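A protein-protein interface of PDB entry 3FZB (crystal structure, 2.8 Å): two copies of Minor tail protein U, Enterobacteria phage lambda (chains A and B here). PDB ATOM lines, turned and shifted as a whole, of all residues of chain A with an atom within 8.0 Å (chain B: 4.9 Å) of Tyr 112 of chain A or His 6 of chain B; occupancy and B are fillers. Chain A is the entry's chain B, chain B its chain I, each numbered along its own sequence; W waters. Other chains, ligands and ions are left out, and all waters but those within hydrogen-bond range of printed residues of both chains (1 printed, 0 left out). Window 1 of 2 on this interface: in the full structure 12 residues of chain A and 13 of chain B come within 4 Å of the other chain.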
ATOM      1  N   GLU A  68      -4.792 -26.079  20.082  1.00  0.00           N
ATOM      2  CA  GLU A  68      -5.030 -25.276  18.894  1.00  0.00           C
ATOM      3  C   GLU A  68      -5.767 -26.067  17.822  1.00  0.00           C
ATOM      4  O   GLU A  68      -5.344 -27.156  17.439  1.00  0.00           O
ATOM      5  CB  GLU A  68      -3.692 -24.770  18.338  1.00  0.00           C
ATOM      6  CG  GLU A  68      -3.808 -23.720  17.249  1.00  0.00           C
ATOM      7  CD  GLU A  68      -2.455 -23.264  16.749  1.00  0.00           C
ATOM      8  OE1 GLU A  68      -1.454 -23.786  17.249  1.00  0.00           O
ATOM      9  OE2 GLU A  68      -2.380 -22.389  15.861  1.00  0.00           O
ATOM     10  N   VAL A  75     -10.843 -18.992   6.695  1.00  0.00           N
ATOM     11  CA  VAL A  75     -12.188 -19.011   7.273  1.00  0.00           C
ATOM     12  C   VAL A  75     -12.345 -17.823   8.232  1.00  0.00           C
ATOM     13  O   VAL A  75     -11.360 -17.254   8.697  1.00  0.00           O
ATOM     14  CB  VAL A  75     -12.418 -20.322   8.021  1.00  0.00           C
ATOM     15  N   PRO A  76     -13.586 -17.415   8.519  1.00  0.00           N
ATOM     16  CA  PRO A  76     -13.777 -16.287   9.437  1.00  0.00           C
ATOM     17  C   PRO A  76     -13.311 -16.699  10.823  1.00  0.00           C
ATOM     18  O   PRO A  76     -13.264 -17.888  11.130  1.00  0.00           O
ATOM     19  CB  PRO A  76     -15.286 -16.057   9.398  1.00  0.00           C
ATOM     20  CG  PRO A  76     -15.659 -16.526   8.029  1.00  0.00           C
ATOM     21  CD  PRO A  76     -14.859 -17.797   7.891  1.00  0.00           C
ATOM     22  N   ASP A  77     -12.972 -15.734  11.667  1.00  0.00           N
ATOM     23  CA  ASP A  77     -12.531 -16.081  13.009  1.00  0.00           C
ATOM     24  C   ASP A  77     -13.677 -16.653  13.796  1.00  0.00           C
ATOM     25  O   ASP A  77     -13.466 -17.381  14.758  1.00  0.00           O
ATOM     26  CB  ASP A  77     -11.963 -14.869  13.742  1.00  0.00           C
ATOM     27  CG  ASP A  77     -10.498 -14.654  13.452  1.00  0.00           C
ATOM     28  OD1 ASP A  77      -9.980 -15.268  12.497  1.00  0.00           O
ATOM     29  OD2 ASP A  77      -9.867 -13.863  14.175  1.00  0.00           O
ATOM     30  N   SER A  78     -14.896 -16.342  13.380  1.00  0.00           N
ATOM     31  CA  SER A  78     -16.061 -16.850  14.088  1.00  0.00           C
ATOM     32  C   SER A  78     -16.367 -18.323  13.826  1.00  0.00           C
ATOM     33  O   SER A  78     -17.064 -18.955  14.610  1.00  0.00           O
ATOM     34  CB  SER A  78     -17.266 -15.986  13.767  1.00  0.00           C
ATOM     35  OG  SER A  78     -16.991 -14.660  14.171  1.00  0.00           O
ATOM     36  N   GLU A  79     -15.850 -18.877  12.732  1.00  0.00           N
ATOM     37  CA  GLU A  79     -16.083 -20.293  12.451  1.00  0.00           C
ATOM     38  C   GLU A  79     -15.147 -21.087  13.371  1.00  0.00           C
ATOM     39  O   GLU A  79     -15.452 -22.204  13.801  1.00  0.00           O
ATOM     40  CB  GLU A  79     -15.771 -20.627  10.986  1.00  0.00           C
ATOM     41  CG  GLU A  79     -16.536 -21.837  10.473  1.00  0.00           C
ATOM     42  CD  GLU A  79     -15.830 -22.557   9.337  1.00  0.00           C
ATOM     43  OE1 GLU A  79     -15.415 -21.892   8.361  1.00  0.00           O
ATOM     44  OE2 GLU A  79     -15.703 -23.800   9.427  1.00  0.00           O
ATOM     45  N   LEU A  80     -13.998 -20.487  13.658  1.00  0.00           N
ATOM     46  CA  LEU A  80     -13.017 -21.092  14.529  1.00  0.00           C
ATOM     47  C   LEU A  80     -13.537 -21.073  15.957  1.00  0.00           C
ATOM     48  O   LEU A  80     -13.381 -22.044  16.687  1.00  0.00           O
ATOM     49  CB  LEU A  80     -11.698 -20.336  14.417  1.00  0.00           C
ATOM     50  CG  LEU A  80     -10.945 -20.657  13.123  1.00  0.00           C
ATOM     51  CD1 LEU A  80      -9.889 -19.623  12.856  1.00  0.00           C
ATOM     52  CD2 LEU A  80     -10.328 -22.031  13.229  1.00  0.00           C
ATOM     53  N   ASP A  81     -14.165 -19.975  16.357  1.00  0.00           N
ATOM     54  CA  ASP A  81     -14.714 -19.876  17.707  1.00  0.00           C
ATOM     55  C   ASP A  81     -15.817 -20.898  17.929  1.00  0.00           C
ATOM     56  O   ASP A  81     -15.919 -21.510  18.988  1.00  0.00           O
ATOM     57  CB  ASP A  81     -15.278 -18.483  17.950  1.00  0.00           C
ATOM     58  CG  ASP A  81     -14.204 -17.463  18.173  1.00  0.00           C
ATOM     59  OD1 ASP A  81     -13.014 -17.826  18.081  1.00  0.00           O
ATOM     60  OD2 ASP A  81     -14.554 -16.296  18.439  1.00  0.00           O
ATOM     61  N   ALA A  82     -16.652 -21.067  16.917  1.00  0.00           N
ATOM     62  CA  ALA A  82     -17.750 -22.008  16.989  1.00  0.00           C
ATOM     63  C   ALA A  82     -17.164 -23.387  17.225  1.00  0.00           C
ATOM     64  O   ALA A  82     -17.572 -24.098  18.142  1.00  0.00           O
ATOM     65  CB  ALA A  82     -18.541 -21.981  15.688  1.00  0.00           C
ATOM     66  N   MET A  84     -14.318 -24.094  18.370  1.00  0.00           N
ATOM     67  CA  MET A  84     -13.701 -24.060  19.691  1.00  0.00           C
ATOM     68  C   MET A  84     -14.742 -24.190  20.802  1.00  0.00           C
ATOM     69  O   MET A  84     -14.574 -24.987  21.723  1.00  0.00           O
ATOM     70  CB  MET A  84     -12.917 -22.758  19.876  1.00  0.00           C
ATOM     71  CG  MET A  84     -11.997 -22.746  21.084  1.00  0.00           C
ATOM     72  SD  MET A  84     -10.674 -23.971  20.942  1.00  0.00           S
ATOM     73  CE  MET A  84      -9.490 -23.103  19.922  1.00  0.00           C
ATOM     74  N   TYR A  89     -13.947 -26.441  24.255  1.00  0.00           N
ATOM     75  CA  TYR A  89     -14.315 -25.854  25.552  1.00  0.00           C
ATOM     76  C   TYR A  89     -14.938 -26.844  26.523  1.00  0.00           C
ATOM     77  O   TYR A  89     -14.536 -26.924  27.682  1.00  0.00           O
ATOM     78  CB  TYR A  89     -15.294 -24.695  25.376  1.00  0.00           C
ATOM     79  CG  TYR A  89     -14.644 -23.338  25.293  1.00  0.00           C
ATOM     80  CD1 TYR A  89     -13.614 -22.981  26.167  1.00  0.00           C
ATOM     81  CD2 TYR A  89     -15.067 -22.394  24.350  1.00  0.00           C
ATOM     82  CE1 TYR A  89     -13.016 -21.717  26.102  1.00  0.00           C
ATOM     83  CE2 TYR A  89     -14.478 -21.130  24.278  1.00  0.00           C
ATOM     84  CZ  TYR A  89     -13.452 -20.802  25.155  1.00  0.00           C
ATOM     85  OH  TYR A  89     -12.848 -19.573  25.071  1.00  0.00           O
ATOM     86  N   GLY A 109      -4.668 -17.511  27.627  1.00  0.00           N
ATOM     87  CA  GLY A 109      -5.176 -16.653  26.574  1.00  0.00           C
ATOM     88  C   GLY A 109      -6.067 -17.346  25.554  1.00  0.00           C
ATOM     89  O   GLY A 109      -6.549 -18.453  25.785  1.00  0.00           O
ATOM     90  N   TYR A 110      -6.277 -16.678  24.424  1.00  0.00           N
ATOM     91  CA  TYR A 110      -7.093 -17.182  23.319  1.00  0.00           C
ATOM     92  C   TYR A 110      -6.592 -16.434  22.085  1.00  0.00           C
ATOM     93  O   TYR A 110      -6.954 -15.278  21.862  1.00  0.00           O
ATOM     94  CB  TYR A 110      -8.565 -16.858  23.576  1.00  0.00           C
ATOM     95  CG  TYR A 110      -9.530 -17.554  22.650  1.00  0.00           C
ATOM     96  CD1 TYR A 110     -10.496 -18.432  23.155  1.00  0.00           C
ATOM     97  CD2 TYR A 110      -9.472 -17.353  21.263  1.00  0.00           C
ATOM     98  CE1 TYR A 110     -11.374 -19.096  22.302  1.00  0.00           C
ATOM     99  CE2 TYR A 110     -10.346 -18.005  20.410  1.00  0.00           C
ATOM    100  CZ  TYR A 110     -11.289 -18.881  20.931  1.00  0.00           C
ATOM    101  OH  TYR A 110     -12.111 -19.575  20.081  1.00  0.00           O
ATOM    102  N   ASP A 111      -5.748 -17.083  21.291  1.00  0.00           N
ATOM    103  CA  ASP A 111      -5.182 -16.426  20.124  1.00  0.00           C
ATOM    104  C   ASP A 111      -5.686 -16.902  18.785  1.00  0.00           C
ATOM    105  O   ASP A 111      -6.279 -17.978  18.643  1.00  0.00           O
ATOM    106  CB  ASP A 111      -3.665 -16.562  20.116  1.00  0.00           C
ATOM    107  CG  ASP A 111      -3.049 -16.217  21.442  1.00  0.00           C
ATOM    108  OD1 ASP A 111      -3.205 -15.067  21.897  1.00  0.00           O
ATOM    109  OD2 ASP A 111      -2.412 -17.109  22.032  1.00  0.00           O
ATOM    110  N   TYR A 112      -5.427 -16.071  17.790  1.00  0.00           N
ATOM    111  CA  TYR A 112      -5.813 -16.362  16.428  1.00  0.00           C
ATOM    112  C   TYR A 112      -4.527 -16.243  15.632  1.00  0.00           C
ATOM    113  O   TYR A 112      -3.850 -15.211  15.677  1.00  0.00           O
ATOM    114  CB  TYR A 112      -6.833 -15.336  15.930  1.00  0.00           C
ATOM    115  CG  TYR A 112      -8.153 -15.376  16.650  1.00  0.00           C
ATOM    116  CD1 TYR A 112      -8.419 -14.516  17.714  1.00  0.00           C
ATOM    117  CD2 TYR A 112      -9.132 -16.289  16.282  1.00  0.00           C
ATOM    118  CE1 TYR A 112      -9.629 -14.565  18.396  1.00  0.00           C
ATOM    119  CE2 TYR A 112     -10.349 -16.352  16.954  1.00  0.00           C
ATOM    120  CZ  TYR A 112     -10.597 -15.491  18.011  1.00  0.00           C
ATOM    121  OH  TYR A 112     -11.802 -15.569  18.681  1.00  0.00           O
ATOM    122  N   ARG A 113      -4.166 -17.316  14.944  1.00  0.00           N
ATOM    123  CA  ARG A 113      -2.967 -17.315  14.130  1.00  0.00           C
ATOM    124  C   ARG A 113      -3.413 -17.810  12.774  1.00  0.00           C
ATOM    125  O   ARG A 113      -4.460 -18.451  12.653  1.00  0.00           O
ATOM    126  CB  ARG A 113      -1.913 -18.275  14.688  1.00  0.00           C
ATOM    127  CG  ARG A 113      -1.468 -18.022  16.118  1.00  0.00           C
ATOM    128  CD  ARG A 113      -0.548 -19.141  16.596  1.00  0.00           C
ATOM    129  NE  ARG A 113      -0.400 -19.179  18.052  1.00  0.00           N
ATOM    130  CZ  ARG A 113       0.222 -20.151  18.714  1.00  0.00           C
ATOM    131  N   ARG A 114      -2.626 -17.512  11.753  1.00  0.00           N
ATOM    132  CA  ARG A 114      -2.961 -17.966  10.421  1.00  0.00           C
ATOM    133  C   ARG A 114      -1.662 -18.275   9.699  1.00  0.00           C
ATOM    134  O   ARG A 114      -0.588 -17.860  10.141  1.00  0.00           O
ATOM    135  CB  ARG A 114      -3.764 -16.892   9.682  1.00  0.00           C
ATOM    136  CG  ARG A 114      -4.646 -17.455   8.589  1.00  0.00           C
ATOM    137  CD  ARG A 114      -5.763 -16.506   8.168  1.00  0.00           C
ATOM    138  NE  ARG A 114      -6.744 -16.286   9.231  1.00  0.00           N
ATOM    139  CZ  ARG A 114      -8.003 -15.897   9.020  1.00  0.00           C
ATOM    140  NH1 ARG A 114      -8.437 -15.689   7.780  1.00  0.00           N
ATOM    141  NH2 ARG A 114      -8.831 -15.717  10.047  1.00  0.00           N
ATOM    142  N   ASP A 116       0.568 -17.312   7.564  1.00  0.00           N
ATOM    143  CA  ASP A 116       1.021 -16.112   6.868  1.00  0.00           C
ATOM    144  C   ASP A 116       2.142 -16.447   5.905  1.00  0.00           C
ATOM    145  O   ASP A 116       2.860 -15.563   5.437  1.00  0.00           O
ATOM    146  CB  ASP A 116       1.492 -15.057   7.874  1.00  0.00           C
ATOM    147  CG  ASP A 116       0.374 -14.582   8.783  1.00  0.00           C
ATOM    148  OD1 ASP A 116      -0.553 -13.888   8.300  1.00  0.00           O
ATOM    149  OD2 ASP A 116       0.420 -14.913   9.989  1.00  0.00           O
ATOM    150  N   TRP A 121      -4.147 -22.399   6.141  1.00  0.00           N
ATOM    151  CA  TRP A 121      -5.000 -22.674   7.289  1.00  0.00           C
ATOM    152  C   TRP A 121      -5.159 -21.466   8.197  1.00  0.00           C
ATOM    153  O   TRP A 121      -4.324 -20.569   8.202  1.00  0.00           O
ATOM    154  CB  TRP A 121      -4.393 -23.817   8.113  1.00  0.00           C
ATOM    155  CG  TRP A 121      -2.963 -23.519   8.527  1.00  0.00           C
ATOM    156  CD1 TRP A 121      -1.825 -23.839   7.838  1.00  0.00           C
ATOM    157  CD2 TRP A 121      -2.541 -22.718   9.638  1.00  0.00           C
ATOM    158  NE1 TRP A 121      -0.728 -23.280   8.445  1.00  0.00           N
ATOM    159  CE2 TRP A 121      -1.140 -22.584   9.551  1.00  0.00           C
ATOM    160  CE3 TRP A 121      -3.212 -22.097  10.698  1.00  0.00           C
ATOM    161  CZ2 TRP A 121      -0.398 -21.850  10.481  1.00  0.00           C
ATOM    162  CZ3 TRP A 121      -2.472 -21.369  11.620  1.00  0.00           C
ATOM    163  CH2 TRP A 121      -1.080 -21.253  11.502  1.00  0.00           C
ATOM    164  N   SER A 122      -6.233 -21.469   8.977  1.00  0.00           N
ATOM    165  CA  SER A 122      -6.522 -20.413   9.935  1.00  0.00           C
ATOM    166  C   SER A 122      -6.664 -21.191  11.242  1.00  0.00           C
ATOM    167  O   SER A 122      -7.113 -22.338  11.225  1.00  0.00           O
ATOM    168  CB  SER A 122      -7.831 -19.705   9.580  1.00  0.00           C
ATOM    169  N   SER A 123      -6.287 -20.591  12.370  1.00  0.00           N
ATOM    170  CA  SER A 123      -6.368 -21.311  13.631  1.00  0.00           C
ATOM    171  C   SER A 123      -6.756 -20.472  14.814  1.00  0.00           C
ATOM    172  O   SER A 123      -6.599 -19.262  14.803  1.00  0.00           O
ATOM    173  CB  SER A 123      -5.019 -21.952  13.950  1.00  0.00           C
ATOM    174  OG  SER A 123      -4.060 -20.958  14.294  1.00  0.00           O
ATOM    175  N   ALA A 124      -7.260 -21.151  15.838  1.00  0.00           N
ATOM    176  CA  ALA A 124      -7.627 -20.532  17.102  1.00  0.00           C
ATOM    177  C   ALA A 124      -6.823 -21.329  18.155  1.00  0.00           C
ATOM    178  O   ALA A 124      -6.723 -22.564  18.076  1.00  0.00           O
ATOM    179  CB  ALA A 124      -9.117 -20.659  17.345  1.00  0.00           C
ATOM    180  N   ASP A 125      -6.241 -20.625  19.123  1.00  0.00           N
ATOM    181  CA  ASP A 125      -5.424 -21.274  20.141  1.00  0.00           C
ATOM    182  C   ASP A 125      -5.929 -21.032  21.573  1.00  0.00           C
ATOM    183  O   ASP A 125      -5.923 -19.899  22.072  1.00  0.00           O
ATOM    184  CB  ASP A 125      -3.981 -20.779  20.002  1.00  0.00           C
ATOM    185  CG  ASP A 125      -2.968 -21.767  20.536  1.00  0.00           C
ATOM    186  OD1 ASP A 125      -3.386 -22.722  21.225  1.00  0.00           O
ATOM    187  OD2 ASP A 125      -1.754 -21.582  20.269  1.00  0.00           O
ATOM    188  N   LEU A 126      -6.363 -22.108  22.225  1.00  0.00           N
ATOM    189  CA  LEU A 126      -6.854 -22.062  23.602  1.00  0.00           C
ATOM    190  C   LEU A 126      -5.722 -22.534  24.520  1.00  0.00           C
ATOM    191  O   LEU A 126      -5.348 -23.707  24.516  1.00  0.00           O
ATOM    192  CB  LEU A 126      -8.054 -22.989  23.756  1.00  0.00           C
ATOM    193  CG  LEU A 126      -8.700 -23.022  25.134  1.00  0.00           C
ATOM    194  CD1 LEU A 126      -9.420 -21.721  25.387  1.00  0.00           C
ATOM    195  CD2 LEU A 126      -9.672 -24.176  25.202  1.00  0.00           C
ATOM    196  N   MET B   4     -19.692 -17.571  20.865  1.00  0.00           N
ATOM    197  CA  MET B   4     -19.311 -17.193  22.256  1.00  0.00           C
ATOM    198  C   MET B   4     -19.381 -15.684  22.484  1.00  0.00           C
ATOM    199  O   MET B   4     -20.460 -15.095  22.408  1.00  0.00           O
ATOM    200  CB  MET B   4     -17.901 -17.720  22.590  1.00  0.00           C
ATOM    201  CG  MET B   4     -16.805 -17.414  21.553  1.00  0.00           C
ATOM    202  SD  MET B   4     -15.424 -16.395  22.176  1.00  0.00           S
ATOM    203  CE  MET B   4     -15.036 -17.239  23.769  1.00  0.00           C
ATOM    204  N   LYS B   5     -18.229 -15.068  22.751  1.00  0.00           N
ATOM    205  CA  LYS B   5     -18.133 -13.627  23.012  1.00  0.00           C
ATOM    206  C   LYS B   5     -17.290 -12.839  21.997  1.00  0.00           C
ATOM    207  O   LYS B   5     -17.611 -11.700  21.675  1.00  0.00           O
ATOM    208  CB  LYS B   5     -17.572 -13.403  24.425  1.00  0.00           C
ATOM    209  CG  LYS B   5     -17.016 -12.010  24.666  1.00  0.00           C
ATOM    210  CD  LYS B   5     -18.105 -10.960  24.702  1.00  0.00           C
ATOM    211  CE  LYS B   5     -18.907 -11.056  25.979  1.00  0.00           C
ATOM    212  NZ  LYS B   5     -19.855  -9.924  26.112  1.00  0.00           N
ATOM    213  N   HIS B   6     -16.209 -13.429  21.504  1.00  0.00           N
ATOM    214  CA  HIS B   6     -15.364 -12.740  20.548  1.00  0.00           C
ATOM    215  C   HIS B   6     -16.057 -12.552  19.207  1.00  0.00           C
ATOM    216  O   HIS B   6     -15.760 -11.608  18.473  1.00  0.00           O
ATOM    217  CB  HIS B   6     -14.065 -13.503  20.366  1.00  0.00           C
ATOM    218  CG  HIS B   6     -13.201 -13.503  21.588  1.00  0.00           C
ATOM    219  ND1 HIS B   6     -11.978 -14.140  21.638  1.00  0.00           N
ATOM    220  CD2 HIS B   6     -13.384 -12.937  22.804  1.00  0.00           C
ATOM    221  CE1 HIS B   6     -11.447 -13.964  22.836  1.00  0.00           C
ATOM    222  NE2 HIS B   6     -12.280 -13.237  23.561  1.00  0.00           N
ATOM    223  N   THR B   7     -16.982 -13.453  18.891  1.00  0.00           N
ATOM    224  CA  THR B   7     -17.730 -13.367  17.641  1.00  0.00           C
ATOM    225  C   THR B   7     -18.648 -12.151  17.701  1.00  0.00           C
ATOM    226  O   THR B   7     -18.804 -11.431  16.723  1.00  0.00           O
ATOM    227  CB  THR B   7     -18.577 -14.632  17.408  1.00  0.00           C
ATOM    228  OG1 THR B   7     -17.714 -15.774  17.353  1.00  0.00           O
ATOM    229  CG2 THR B   7     -19.348 -14.527  16.099  1.00  0.00           C
ATOM    230  N   GLU B   8     -19.249 -11.932  18.861  1.00  0.00           N
ATOM    231  CA  GLU B   8     -20.129 -10.793  19.054  1.00  0.00           C
ATOM    232  C   GLU B   8     -19.294  -9.512  19.009  1.00  0.00           C
ATOM    233  O   GLU B   8     -19.595  -8.596  18.245  1.00  0.00           O
ATOM    234  CB  GLU B   8     -20.849 -10.909  20.399  1.00  0.00           C
ATOM    235  CG  GLU B   8     -21.570 -12.239  20.601  1.00  0.00           C
ATOM    236  CD  GLU B   8     -22.465 -12.247  21.838  1.00  0.00           C
ATOM    237  OE1 GLU B   8     -21.939 -12.146  22.967  1.00  0.00           O
ATOM    238  OE2 GLU B   8     -23.704 -12.350  21.680  1.00  0.00           O
ATOM    239  N   LEU B   9     -18.243  -9.456  19.828  1.00  0.00           N
ATOM    240  CA  LEU B   9     -17.352  -8.296  19.867  1.00  0.00           C
ATOM    241  C   LEU B   9     -17.001  -7.890  18.443  1.00  0.00           C
ATOM    242  O   LEU B   9     -17.339  -6.796  17.999  1.00  0.00           O
ATOM    243  CB  LEU B   9     -16.065  -8.623  20.638  1.00  0.00           C
ATOM    244  CG  LEU B   9     -15.997  -8.402  22.155  1.00  0.00           C
ATOM    245  CD1 LEU B   9     -14.848  -9.195  22.763  1.00  0.00           C
ATOM    246  CD2 LEU B   9     -15.807  -6.926  22.435  1.00  0.00           C
ATOM    247  N   ARG B  10     -16.332  -8.784  17.726  1.00  0.00           N
ATOM    248  CA  ARG B  10     -15.946  -8.498  16.355  1.00  0.00           C
ATOM    249  C   ARG B  10     -17.142  -8.078  15.532  1.00  0.00           C
ATOM    250  O   ARG B  10     -17.095  -7.082  14.819  1.00  0.00           O
ATOM    251  CB  ARG B  10     -15.311  -9.720  15.699  1.00  0.00           C
ATOM    252  CG  ARG B  10     -13.904 -10.053  16.169  1.00  0.00           C
ATOM    253  CD  ARG B  10     -13.318 -11.108  15.254  1.00  0.00           C
ATOM    254  NE  ARG B  10     -14.113 -12.332  15.264  1.00  0.00           N
ATOM    255  CZ  ARG B  10     -13.999 -13.286  16.178  1.00  0.00           C
ATOM    256  NH1 ARG B  10     -13.112 -13.165  17.159  1.00  0.00           N
ATOM    257  NH2 ARG B  10     -14.784 -14.353  16.127  1.00  0.00           N
ATOM    258  N   ALA B  11     -18.219  -8.845  15.636  1.00  0.00           N
ATOM    259  CA  ALA B  11     -19.431  -8.575  14.883  1.00  0.00           C
ATOM    260  C   ALA B  11     -19.923  -7.162  15.093  1.00  0.00           C
ATOM    261  O   ALA B  11     -20.106  -6.421  14.136  1.00  0.00           O
ATOM    262  CB  ALA B  11     -20.500  -9.557  15.268  1.00  0.00           C
ATOM    263  N   LEU B  46      -9.003  -9.554  16.911  1.00  0.00           N
ATOM    264  CA  LEU B  46      -8.478  -9.346  18.255  1.00  0.00           C
ATOM    265  C   LEU B  46      -7.095  -9.999  18.403  1.00  0.00           C
ATOM    266  O   LEU B  46      -6.808 -11.022  17.781  1.00  0.00           O
ATOM    267  CB  LEU B  46      -9.405  -9.964  19.311  1.00  0.00           C
ATOM    268  CG  LEU B  46     -10.882  -9.599  19.445  1.00  0.00           C
ATOM    269  CD1 LEU B  46     -11.486 -10.440  20.554  1.00  0.00           C
ATOM    270  CD2 LEU B  46     -11.054  -8.128  19.742  1.00  0.00           C
ATOM    271  N   ALA B  49      -5.834 -11.626  23.445  1.00  0.00           N
ATOM    272  CA  ALA B  49      -6.984 -11.843  24.324  1.00  0.00           C
ATOM    273  C   ALA B  49      -6.368 -12.606  25.475  1.00  0.00           C
ATOM    274  O   ALA B  49      -5.537 -13.476  25.244  1.00  0.00           O
ATOM    275  CB  ALA B  49      -8.018 -12.700  23.640  1.00  0.00           C
ATOM    276  N   TYR B 132     -13.614  -7.275  29.197  1.00  0.00           N
ATOM    277  CA  TYR B 132     -14.955  -7.837  29.137  1.00  0.00           C
ATOM    278  C   TYR B 132     -15.078  -9.146  29.893  1.00  0.00           C
ATOM    279  O   TYR B 132     -14.085  -9.703  30.361  1.00  0.00           O
ATOM    280  CB  TYR B 132     -15.318  -8.071  27.673  1.00  0.00           C
ATOM    281  CG  TYR B 132     -14.269  -8.879  26.927  1.00  0.00           C
ATOM    282  CD1 TYR B 132     -14.441 -10.244  26.690  1.00  0.00           C
ATOM    283  CD2 TYR B 132     -13.084  -8.279  26.487  1.00  0.00           C
ATOM    284  CE1 TYR B 132     -13.461 -10.994  26.031  1.00  0.00           C
ATOM    285  CE2 TYR B 132     -12.093  -9.021  25.830  1.00  0.00           C
ATOM    286  CZ  TYR B 132     -12.290 -10.376  25.606  1.00  0.00           C
ATOM    287  OH  TYR B 132     -11.311 -11.109  24.973  1.00  0.00           O
ATOM    288  N   MET B 134     -16.301 -13.141  29.802  1.00  0.00           N
ATOM    289  CA  MET B 134     -16.520 -14.259  28.899  1.00  0.00           C
ATOM    290  C   MET B 134     -17.753 -15.035  29.348  1.00  0.00           C
ATOM    291  O   MET B 134     -18.725 -15.091  28.561  1.00  0.00           O
ATOM    292  CB  MET B 134     -15.290 -15.170  28.902  1.00  0.00           C
ATOM    293  CG  MET B 134     -15.127 -16.017  27.655  1.00  0.00           C
ATOM    294  SD  MET B 134     -14.613 -15.093  26.191  1.00  0.00           S
ATOM    295  CE  MET B 134     -12.841 -15.360  26.210  1.00  0.00           C
ATOM    296  OXT MET B 134     -17.730 -15.566  30.482  1.00  0.00           O
HETATM  297  O   HOH W   1      -2.359 -14.029  25.081  1.00  0.00           O
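Of chain B, only His 6 (3.3 Å), Arg 10 (3.1 Å) and Leu 46 (3.8 Å) come within 4 Å of Tyr 112 of chain A.
Of the printed residues of chain B, Tyr 110 of chain A touches Ala 49.
Printed residues of chain A within 4 Å of Leu 46 of chain B: Tyr 112.
Ala 11 of chain B touches none of the printed residues of chain A.
Val 75 of chain A touches none of the printed residues of chain B.
The nearest residue of chain A that does not touch His 6 of chain B is Tyr 110 of chain A (4.1 Å).
Hydrophobic or aromatic side chains of chain A that line the printed part of chain B: Tyr 89 and Tyr 112.
Of the 12 printed residues of chain B, 6 touch a printed residue of chain A.
Among the printed residues, Asp or Glu carboxylates within 4 Å of a Lys or Arg side-chain nitrogen of the other chain: Asp 81 of chain A with Arg 10 of chain B (3.0 Å).
The side-chain hydroxyl (OG) of Ser 78 of chain A lies close to the side-chain hydroxyl (OG1) of Thr 7 of chain B, 3.4 Å away.
OG of Ser 78 of chain A is in hydrogen-bond range of NH2 of Arg 10 of chain B (3.0 Å).
The side-chain hydroxyl of Thr 7 of chain B is in hydrogen-bond range of the side-chain carboxylate of Asp 81 of chain A.
The side-chain carboxylate of Asp 81 of chain A is in salt-bridge range of the guanidinium group of Arg 10 of chain B (3.0 Å).
The backbone NH (N) of Tyr 110 of chain A lies within hydrogen-bond range of the backbone carbonyl oxygen (O) of Ala 49 of chain B (3.4 Å).
The side-chain hydroxyl (OH) of Tyr 112 of chain A sits at hydrogen-bond distance from a ring nitrogen (ND1) of His 6 of chain B (3.3 Å).
The side-chain hydroxyl of Tyr 112 of chain A is in hydrogen-bond range of the guanidinium group of Arg 10 of chain B.
No position is printed for both chains.
Water W1 lies within hydrogen-bond range of O of Ala 49 of chain B (3.2 Å) and OD1 of Asp 111 of chain A (3.5 Å).
OD1 of Asp 77 of chain A is in salt-bridge range of NH2 of Arg 114 of chain A.
OD1 of Asp 81 of chain A is in hydrogen-bond range of OH of Tyr 110 of chain A, at 2.8 Å.
OD1 of Asp 81 of chain A lies within hydrogen-bond range of OH of Tyr 112 of chain A.
N of Tyr 89 of chain A is in hydrogen-bond range of O of Met 84 of chain A (3.0 Å).
O of His 6 of chain B is in hydrogen-bond range of NH1 of Arg 10 of chain B (3.3 Å).
NE2 of His 6 of chain B sits at hydrogen-bond distance from OH of Tyr 132 of chain B (2.7 Å).
Among the printed residues, pairs that only touch across the chains: Asp 77 of chain A with Arg 10 of chain B (3.5 Å), Asp 81 of chain A with Met 4 of chain B (3.8 Å), Asp 81 of chain A with His 6 of chain B (3.4 Å), Tyr 89 of chain A with Met 4 of chain B (3.5 Å), Gly 109 of chain A with Ala 49 of chain B (3.5 Å) and Tyr 112 of chain A with Leu 46 of chain B (3.8 Å).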
